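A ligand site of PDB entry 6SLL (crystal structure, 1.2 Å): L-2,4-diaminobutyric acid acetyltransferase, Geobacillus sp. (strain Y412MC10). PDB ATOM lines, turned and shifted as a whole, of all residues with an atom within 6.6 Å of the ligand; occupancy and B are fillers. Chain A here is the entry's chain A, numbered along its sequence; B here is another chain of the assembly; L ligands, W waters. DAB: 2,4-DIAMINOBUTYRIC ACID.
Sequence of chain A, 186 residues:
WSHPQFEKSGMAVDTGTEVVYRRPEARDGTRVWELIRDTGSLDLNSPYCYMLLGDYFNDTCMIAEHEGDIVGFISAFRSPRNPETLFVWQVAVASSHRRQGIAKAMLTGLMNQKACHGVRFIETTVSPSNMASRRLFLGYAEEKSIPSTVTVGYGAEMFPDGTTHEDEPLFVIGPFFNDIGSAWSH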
ATOM      1  N   ILE A  36     -14.364  -2.999  25.725  1.00  0.00           N
ATOM      2  CA  ILE A  36     -15.508  -3.860  25.534  1.00  0.00           C
ATOM      3  C   ILE A  36     -15.870  -4.600  26.836  1.00  0.00           C
ATOM      4  O   ILE A  36     -17.043  -4.693  27.196  1.00  0.00           O
ATOM      5  CB  ILE A  36     -15.255  -4.765  24.369  1.00  0.00           C
ATOM      6  CG1 ILE A  36     -15.111  -3.905  23.122  1.00  0.00           C
ATOM      7  CG2 ILE A  36     -16.373  -5.772  24.184  1.00  0.00           C
ATOM      8  CD1 ILE A  36     -14.595  -4.686  22.056  1.00  0.00           C
ATOM      9  N   SER A  41     -21.663  -5.509  28.896  1.00  0.00           N
ATOM     10  CA  SER A  41     -22.864  -5.774  28.130  1.00  0.00           C
ATOM     11  C   SER A  41     -22.642  -6.202  26.648  1.00  0.00           C
ATOM     12  O   SER A  41     -23.603  -6.194  25.904  1.00  0.00           O
ATOM     13  CB  SER A  41     -23.792  -4.597  28.201  1.00  0.00           C
ATOM     14  OG  SER A  41     -23.159  -3.471  27.600  1.00  0.00           O
ATOM     15  N   LEU A  42     -21.503  -6.313  26.155  1.00  0.00           N
ATOM     16  CA  LEU A  42     -21.139  -6.844  24.848  1.00  0.00           C
ATOM     17  C   LEU A  42     -20.576  -8.175  25.120  1.00  0.00           C
ATOM     18  O   LEU A  42     -20.007  -8.497  26.137  1.00  0.00           O
ATOM     19  CB  LEU A  42     -20.203  -5.902  24.157  1.00  0.00           C
ATOM     20  CG  LEU A  42     -20.688  -4.618  23.659  1.00  0.00           C
ATOM     21  CD1 LEU A  42     -19.605  -3.642  23.269  1.00  0.00           C
ATOM     22  CD2 LEU A  42     -21.561  -4.809  22.414  1.00  0.00           C
ATOM     23  N   ASP A  43     -20.648  -8.991  24.071  1.00  0.00           N
ATOM     24  CA  ASP A  43     -20.007 -10.346  24.082  1.00  0.00           C
ATOM     25  C   ASP A  43     -18.498 -10.105  24.046  1.00  0.00           C
ATOM     26  O   ASP A  43     -18.007  -9.510  23.114  1.00  0.00           O
ATOM     27  CB  ASP A  43     -20.562 -11.161  22.877  1.00  0.00           C
ATOM     28  CG  ASP A  43     -21.930 -11.765  23.105  1.00  0.00           C
ATOM     29  OD1 ASP A  43     -22.062 -12.589  24.031  1.00  0.00           O
ATOM     30  OD2 ASP A  43     -22.889 -11.372  22.425  1.00  0.00           O
ATOM     31  N   LEU A  44     -17.765 -10.503  25.018  1.00  0.00           N
ATOM     32  CA  LEU A  44     -16.378 -10.187  25.049  1.00  0.00           C
ATOM     33  C   LEU A  44     -15.603 -11.271  24.274  1.00  0.00           C
ATOM     34  O   LEU A  44     -15.666 -12.460  24.628  1.00  0.00           O
ATOM     35  CB  LEU A  44     -15.909 -10.134  26.496  1.00  0.00           C
ATOM     36  CG  LEU A  44     -14.460  -9.717  26.708  1.00  0.00           C
ATOM     37  CD1 LEU A  44     -14.124  -8.353  26.127  1.00  0.00           C
ATOM     38  CD2 LEU A  44     -14.139  -9.768  28.167  1.00  0.00           C
ATOM     39  N   ASN A  45     -14.829 -10.892  23.285  1.00  0.00           N
ATOM     40  CA  ASN A  45     -13.901 -11.811  22.608  1.00  0.00           C
ATOM     41  C   ASN A  45     -12.528 -11.770  23.250  1.00  0.00           C
ATOM     42  O   ASN A  45     -12.319 -11.002  24.188  1.00  0.00           O
ATOM     43  CB  ASN A  45     -13.881 -11.479  21.113  1.00  0.00           C
ATOM     44  CG  ASN A  45     -15.248 -11.637  20.535  1.00  0.00           C
ATOM     45  OD1 ASN A  45     -15.794 -12.769  20.477  1.00  0.00           O
ATOM     46  ND2 ASN A  45     -15.920 -10.577  20.162  1.00  0.00           N
ATOM     47  N   TYR A  50      -9.100  -8.800  19.147  1.00  0.00           N
ATOM     48  CA  TYR A  50      -9.027  -7.351  18.900  1.00  0.00           C
ATOM     49  C   TYR A  50      -7.695  -6.979  18.294  1.00  0.00           C
ATOM     50  O   TYR A  50      -7.681  -5.998  17.517  1.00  0.00           O
ATOM     51  CB  TYR A  50      -9.389  -6.579  20.205  1.00  0.00           C
ATOM     52  CG  TYR A  50     -10.797  -6.896  20.647  1.00  0.00           C
ATOM     53  CD1 TYR A  50     -11.869  -6.431  19.962  1.00  0.00           C
ATOM     54  CD2 TYR A  50     -11.053  -7.756  21.705  1.00  0.00           C
ATOM     55  CE1 TYR A  50     -13.204  -6.794  20.291  1.00  0.00           C
ATOM     56  CE2 TYR A  50     -12.323  -8.135  22.033  1.00  0.00           C
ATOM     57  CZ  TYR A  50     -13.409  -7.652  21.331  1.00  0.00           C
ATOM     58  OH  TYR A  50     -14.691  -8.062  21.661  1.00  0.00           O
ATOM     59  N   PHE A  87     -20.589  -5.593   7.375  1.00  0.00           N
ATOM     60  CA  PHE A  87     -21.102  -6.103   8.606  1.00  0.00           C
ATOM     61  C   PHE A  87     -20.462  -5.331   9.751  1.00  0.00           C
ATOM     62  O   PHE A  87     -19.249  -5.313   9.890  1.00  0.00           O
ATOM     63  CB  PHE A  87     -20.792  -7.596   8.791  1.00  0.00           C
ATOM     64  CG  PHE A  87     -21.421  -8.154  10.028  1.00  0.00           C
ATOM     65  CD1 PHE A  87     -22.762  -8.515  10.018  1.00  0.00           C
ATOM     66  CD2 PHE A  87     -20.687  -8.307  11.194  1.00  0.00           C
ATOM     67  CE1 PHE A  87     -23.314  -9.011  11.179  1.00  0.00           C
ATOM     68  CE2 PHE A  87     -21.347  -8.865  12.327  1.00  0.00           C
ATOM     69  CZ  PHE A  87     -22.648  -9.167  12.270  1.00  0.00           C
ATOM     70  N   VAL A  88     -21.311  -4.702  10.597  1.00  0.00           N
ATOM     71  CA  VAL A  88     -20.866  -4.023  11.807  1.00  0.00           C
ATOM     72  C   VAL A  88     -21.008  -4.958  12.973  1.00  0.00           C
ATOM     73  O   VAL A  88     -22.138  -5.440  13.237  1.00  0.00           O
ATOM     74  CB  VAL A  88     -21.599  -2.698  12.003  1.00  0.00           C
ATOM     75  CG1 VAL A  88     -21.112  -2.071  13.324  1.00  0.00           C
ATOM     76  CG2 VAL A  88     -21.349  -1.789  10.832  1.00  0.00           C
ATOM     77  N   TRP A  89     -19.910  -5.337  13.556  1.00  0.00           N
ATOM     78  CA  TRP A  89     -19.856  -6.340  14.597  1.00  0.00           C
ATOM     79  C   TRP A  89     -20.105  -5.782  15.986  1.00  0.00           C
ATOM     80  O   TRP A  89     -21.123  -6.106  16.602  1.00  0.00           O
ATOM     81  CB  TRP A  89     -18.520  -7.072  14.471  1.00  0.00           C
ATOM     82  CG  TRP A  89     -18.312  -8.241  15.382  1.00  0.00           C
ATOM     83  CD1 TRP A  89     -19.083  -8.742  16.362  1.00  0.00           C
ATOM     84  CD2 TRP A  89     -17.147  -9.052  15.397  1.00  0.00           C
ATOM     85  NE1 TRP A  89     -18.443  -9.793  16.953  1.00  0.00           N
ATOM     86  CE2 TRP A  89     -17.269 -10.032  16.367  1.00  0.00           C
ATOM     87  CE3 TRP A  89     -15.977  -9.082  14.553  1.00  0.00           C
ATOM     88  CZ2 TRP A  89     -16.295 -10.980  16.600  1.00  0.00           C
ATOM     89  CZ3 TRP A  89     -15.043 -10.063  14.788  1.00  0.00           C
ATOM     90  CH2 TRP A  89     -15.213 -10.999  15.799  1.00  0.00           C
ATOM     91  N   GLN A  90     -19.179  -4.955  16.503  1.00  0.00           N
ATOM     92  CA  GLN A  90     -19.357  -4.373  17.818  1.00  0.00           C
ATOM     93  C   GLN A  90     -19.205  -2.871  17.771  1.00  0.00           C
ATOM     94  O   GLN A  90     -18.279  -2.342  17.091  1.00  0.00           O
ATOM     95  CB  GLN A  90     -18.390  -4.957  18.831  1.00  0.00           C
ATOM     96  CG  GLN A  90     -18.684  -6.415  19.122  1.00  0.00           C
ATOM     97  CD  GLN A  90     -17.785  -7.053  20.152  1.00  0.00           C
ATOM     98  OE1 GLN A  90     -16.553  -7.043  20.062  1.00  0.00           O
ATOM     99  NE2 GLN A  90     -18.414  -7.650  21.132  1.00  0.00           N
ATOM    100  N   VAL A  91     -20.033  -2.159  18.493  1.00  0.00           N
ATOM    101  CA  VAL A  91     -19.923  -0.734  18.714  1.00  0.00           C
ATOM    102  C   VAL A  91     -19.948  -0.467  20.212  1.00  0.00           C
ATOM    103  O   VAL A  91     -20.871  -0.946  20.895  1.00  0.00           O
ATOM    104  CB  VAL A  91     -21.058   0.081  18.042  1.00  0.00           C
ATOM    105  CG1 VAL A  91     -20.815   1.567  18.210  1.00  0.00           C
ATOM    106  CG2 VAL A  91     -21.282  -0.296  16.603  1.00  0.00           C
ATOM    107  N   THR A 124     -26.090  -5.658  10.722  1.00  0.00           N
ATOM    108  CA  THR A 124     -25.627  -5.717  12.059  1.00  0.00           C
ATOM    109  C   THR A 124     -26.730  -6.430  12.885  1.00  0.00           C
ATOM    110  O   THR A 124     -27.875  -6.407  12.429  1.00  0.00           O
ATOM    111  CB  THR A 124     -25.355  -4.301  12.643  1.00  0.00           C
ATOM    112  OG1 THR A 124     -24.607  -4.375  13.819  1.00  0.00           O
ATOM    113  CG2 THR A 124     -26.593  -3.497  12.842  1.00  0.00           C
ATOM    114  N   THR A 125     -26.421  -6.955  14.041  1.00  0.00           N
ATOM    115  CA  THR A 125     -27.474  -7.503  14.899  1.00  0.00           C
ATOM    116  C   THR A 125     -27.654  -6.648  16.116  1.00  0.00           C
ATOM    117  O   THR A 125     -26.670  -6.122  16.662  1.00  0.00           O
ATOM    118  CB  THR A 125     -27.273  -8.976  15.260  1.00  0.00           C
ATOM    119  OG1 THR A 125     -26.164  -9.136  16.146  1.00  0.00           O
ATOM    120  CG2 THR A 125     -27.070  -9.855  14.059  1.00  0.00           C
ATOM    121  N   VAL A 126     -28.915  -6.474  16.518  1.00  0.00           N
ATOM    122  CA  VAL A 126     -29.178  -5.591  17.647  1.00  0.00           C
ATOM    123  C   VAL A 126     -30.263  -6.298  18.547  1.00  0.00           C
ATOM    124  O   VAL A 126     -31.422  -6.415  18.148  1.00  0.00           O
ATOM    125  CB  VAL A 126     -29.771  -4.226  17.197  1.00  0.00           C
ATOM    126  CG1 VAL A 126     -29.954  -3.370  18.466  1.00  0.00           C
ATOM    127  CG2 VAL A 126     -28.860  -3.519  16.200  1.00  0.00           C
ATOM    128  N   SER A 127     -29.837  -6.699  19.716  1.00  0.00           N
ATOM    129  CA  SER A 127     -30.775  -7.369  20.608  1.00  0.00           C
ATOM    130  C   SER A 127     -31.848  -6.375  21.074  1.00  0.00           C
ATOM    131  O   SER A 127     -31.604  -5.167  21.215  1.00  0.00           O
ATOM    132  CB  SER A 127     -30.001  -7.957  21.801  1.00  0.00           C
ATOM    133  OG  SER A 127     -29.136  -8.970  21.428  1.00  0.00           O
ATOM    134  N   SER A 133     -28.490   1.168  20.770  1.00  0.00           N
ATOM    135  CA  SER A 133     -27.964   0.634  19.508  1.00  0.00           C
ATOM    136  C   SER A 133     -29.002   0.638  18.421  1.00  0.00           C
ATOM    137  O   SER A 133     -28.699   0.969  17.274  1.00  0.00           O
ATOM    138  CB  SER A 133     -27.474  -0.744  19.735  1.00  0.00           C
ATOM    139  OG  SER A 133     -27.011  -1.325  18.552  1.00  0.00           O
ATOM    140  N   PHE A 137     -28.605   2.754  14.709  1.00  0.00           N
ATOM    141  CA  PHE A 137     -28.710   2.250  13.355  1.00  0.00           C
ATOM    142  C   PHE A 137     -29.980   2.732  12.649  1.00  0.00           C
ATOM    143  O   PHE A 137     -29.912   3.085  11.470  1.00  0.00           O
ATOM    144  CB  PHE A 137     -28.564   0.711  13.339  1.00  0.00           C
ATOM    145  CG  PHE A 137     -27.174   0.288  13.640  1.00  0.00           C
ATOM    146  CD1 PHE A 137     -26.198   0.378  12.626  1.00  0.00           C
ATOM    147  CD2 PHE A 137     -26.750  -0.185  14.833  1.00  0.00           C
ATOM    148  CE1 PHE A 137     -24.895   0.018  12.879  1.00  0.00           C
ATOM    149  CE2 PHE A 137     -25.433  -0.543  15.086  1.00  0.00           C
ATOM    150  CZ  PHE A 137     -24.511  -0.415  14.101  1.00  0.00           C
ATOM    151  N   HIS A 165     -28.971 -15.778  26.507  1.00  0.00           N
ATOM    152  CA  HIS A 165     -28.617 -14.699  25.578  1.00  0.00           C
ATOM    153  C   HIS A 165     -29.853 -14.160  24.948  1.00  0.00           C
ATOM    154  O   HIS A 165     -30.789 -14.957  24.603  1.00  0.00           O
ATOM    155  CB  HIS A 165     -27.657 -15.200  24.551  1.00  0.00           C
ATOM    156  CG  HIS A 165     -26.824 -14.128  23.858  1.00  0.00           C
ATOM    157  ND1 HIS A 165     -27.341 -13.269  22.935  1.00  0.00           N
ATOM    158  CD2 HIS A 165     -25.519 -13.841  24.004  1.00  0.00           C
ATOM    159  CE1 HIS A 165     -26.360 -12.501  22.490  1.00  0.00           C
ATOM    160  NE2 HIS A 165     -25.240 -12.830  23.117  1.00  0.00           N
ATOM    161  N   GLU A 168     -30.554 -12.023  18.627  1.00  0.00           N
ATOM    162  CA  GLU A 168     -29.736 -11.084  17.870  1.00  0.00           C
ATOM    163  C   GLU A 168     -30.332 -10.940  16.500  1.00  0.00           C
ATOM    164  O   GLU A 168     -29.798 -11.460  15.509  1.00  0.00           O
ATOM    165  CB  GLU A 168     -28.315 -11.597  17.810  1.00  0.00           C
ATOM    166  CG  GLU A 168     -27.576 -11.535  19.112  1.00  0.00           C
ATOM    167  CD  GLU A 168     -26.933 -10.188  19.462  1.00  0.00           C
ATOM    168  OE1 GLU A 168     -27.043  -9.242  18.663  1.00  0.00           O
ATOM    169  OE2 GLU A 168     -26.313 -10.110  20.538  1.00  0.00           O
ATOM    170  N   SER B  46     -16.147 -15.245  21.978  1.00  0.00           N
ATOM    171  CA  SER B  46     -17.549 -15.407  22.325  1.00  0.00           C
ATOM    172  C   SER B  46     -18.230 -16.409  21.421  1.00  0.00           C
ATOM    173  O   SER B  46     -17.806 -16.633  20.284  1.00  0.00           O
ATOM    174  CB  SER B  46     -18.304 -14.079  22.233  1.00  0.00           C
ATOM    175  OG  SER B  46     -18.400 -13.636  20.897  1.00  0.00           O
ATOM    176  N   TYR B  48     -20.912 -15.905  19.859  1.00  0.00           N
ATOM    177  CA  TYR B  48     -21.310 -15.074  18.705  1.00  0.00           C
ATOM    178  C   TYR B  48     -20.186 -15.039  17.670  1.00  0.00           C
ATOM    179  O   TYR B  48     -20.484 -15.079  16.468  1.00  0.00           O
ATOM    180  CB  TYR B  48     -21.646 -13.653  19.223  1.00  0.00           C
ATOM    181  CG  TYR B  48     -22.241 -12.739  18.198  1.00  0.00           C
ATOM    182  CD1 TYR B  48     -21.401 -12.009  17.349  1.00  0.00           C
ATOM    183  CD2 TYR B  48     -23.573 -12.526  18.083  1.00  0.00           C
ATOM    184  CE1 TYR B  48     -21.912 -11.147  16.447  1.00  0.00           C
ATOM    185  CE2 TYR B  48     -24.125 -11.681  17.175  1.00  0.00           C
ATOM    186  CZ  TYR B  48     -23.324 -10.937  16.349  1.00  0.00           C
ATOM    187  OH  TYR B  48     -23.781 -10.025  15.440  1.00  0.00           O
ATOM    188  N   CYS B  49     -18.931 -14.903  18.087  1.00  0.00           N
ATOM    189  CA  CYS B  49     -17.814 -14.930  17.150  1.00  0.00           C
ATOM    190  C   CYS B  49     -17.849 -16.138  16.283  1.00  0.00           C
ATOM    191  O   CYS B  49     -17.621 -16.075  15.068  1.00  0.00           O
ATOM    192  CB  CYS B  49     -16.517 -14.807  17.935  1.00  0.00           C
ATOM    193  SG  CYS B  49     -15.019 -14.765  16.922  1.00  0.00           S
ATOM    194  N   LEU B  52     -20.472 -15.962  13.694  1.00  0.00           N
ATOM    195  CA  LEU B  52     -20.020 -15.122  12.584  1.00  0.00           C
ATOM    196  C   LEU B  52     -19.126 -15.836  11.657  1.00  0.00           C
ATOM    197  O   LEU B  52     -19.225 -15.673  10.417  1.00  0.00           O
ATOM    198  CB  LEU B  52     -19.286 -13.886  13.002  1.00  0.00           C
ATOM    199  CG  LEU B  52     -19.976 -12.840  13.696  1.00  0.00           C
ATOM    200  CD1 LEU B  52     -19.031 -11.633  13.896  1.00  0.00           C
ATOM    201  CD2 LEU B  52     -21.222 -12.363  12.927  1.00  0.00           C
HETATM  202  N   DAB L   1     -23.843  -9.048  21.029  1.00  0.00           N
HETATM  203  CA  DAB L   1     -22.971  -9.159  19.838  1.00  0.00           C
HETATM  204  C   DAB L   1     -21.521  -8.859  20.228  1.00  0.00           C
HETATM  205  O   DAB L   1     -21.329  -8.213  21.269  1.00  0.00           O
HETATM  206  CB  DAB L   1     -23.448  -8.366  18.631  1.00  0.00           C
HETATM  207  CG  DAB L   1     -23.309  -6.929  18.815  1.00  0.00           C
HETATM  208  ND  DAB L   1     -23.862  -6.238  17.581  1.00  0.00           N
HETATM  209  OXT DAB L   1     -20.662  -9.195  19.414  1.00  0.00           O
HETATM  210  O   HOH W   1     -22.668  -3.585  18.681  1.00  0.00           O
HETATM  211  O   HOH W   2     -24.486  -9.170  24.001  1.00  0.00           O
HETATM  212  O   HOH W   3     -18.771 -10.977  19.691  1.00  0.00           O
HETATM  213  O   HOH W   4     -26.152  -4.097  18.908  1.00  0.00           O
HETATM  214  O   HOH W   5     -24.642  -3.526  16.543  1.00  0.00           O
HETATM  215  O   HOH W   6     -23.591  -7.223  14.902  1.00  0.00           O
HETATM  216  O   HOH W   7     -24.733  -6.685  22.240  1.00  0.00           O
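Merely in contact with the ligand: Tyr 48 of chain B and Leu 42.
Hydrophobic or aromatic side chains within 4 Å of the ligand: Leu 42, Trp 89 and Tyr 48 of chain B.
Seven residues have an atom within 4 Å of the ligand: Leu 42, Asp 43, Trp 89, Gln 90, Thr 125, Glu 168 and Tyr 48 of chain B.
Along chain A the residues within 4 Å of the ligand span positions 42 to 168.
OG of Ser 127 sits at hydrogen-bond distance from OE2 of Glu 168 (3.2 Å).
The side-chain hydroxyl (OG1) of Thr 125 lies within hydrogen-bond range of the side-chain carboxylate (OE1) of Glu 168, 2.7 Å away.
NE2 of His 165 sits at hydrogen-bond distance from OD2 of Asp 43 (2.9 Å).
The side-chain amide oxygen (OE1) of Gln 90 is in hydrogen-bond range of the side-chain hydroxyl (OH) of Tyr 50 (2.7 Å).
The backbone carbonyl oxygen (O) of Asp 43 is in hydrogen-bond range of the side-chain amide nitrogen (NE2) of Gln 90 (2.7 Å).
The side-chain hydroxyl of Thr 125 lies within hydrogen-bond range of the side-chain hydroxyl of Tyr 48 of chain B (2.6 Å).
Water W3 lies within hydrogen-bond range of OXT of the ligand, ND2 of Asn 45, OG of Ser 46 of chain B and NE1 of Trp 89.
Water W6 lies within hydrogen-bond range of the backbone carbonyl oxygen of Val 88 (2.8 Å), the side-chain hydroxyl of Tyr 48 of chain B (2.9 Å), a nitrogen (ND) of the ligand (2.9 Å), the backbone NH of Thr 125 (3.0 Å), the backbone carbonyl oxygen of Trp 89 (3.2 Å) and the side-chain hydroxyl of Thr 124 (3.2 Å).
Water W5 lies within hydrogen-bond range of OG1 of Thr 124 (2.9 Å), ND of the ligand (3.0 Å) and O of Thr 125 (3.3 Å).
Water W2 lies within hydrogen-bond range of N of the ligand and OD2 of Asp 43.
Water W1 lies within hydrogen-bond range of N of Val 91 and ND of the ligand.
Water W4 lies within hydrogen-bond range of OG of Ser 133 (2.9 Å), O of Thr 125 (3.1 Å) and ND of the ligand (3.4 Å).
N of Asp 43 is in hydrogen-bond range of O of the ligand (3.0 Å).
The indole nitrogen of Trp 89 sits at hydrogen-bond distance from an oxygen (OXT) of the ligand (3.4 Å).
The side-chain carboxylate (OE2) of Glu 168 is in salt-bridge range of a nitrogen (N) of the ligand (2.7 Å).
ND of the ligand sits at hydrogen-bond distance from O of Thr 125 (3.0 Å).
The side-chain amide nitrogen (NE2) of Gln 90 lies within hydrogen-bond range of an oxygen (O) of the ligand (3.0 Å).
The backbone carbonyl oxygen of Trp 89 is in hydrogen-bond range of a nitrogen (ND) of the ligand, at 2.9 Å.
A nitrogen (N) of the ligand lies within salt-bridge range of the side-chain carboxylate (OD2) of Asp 43, 2.9 Å away.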
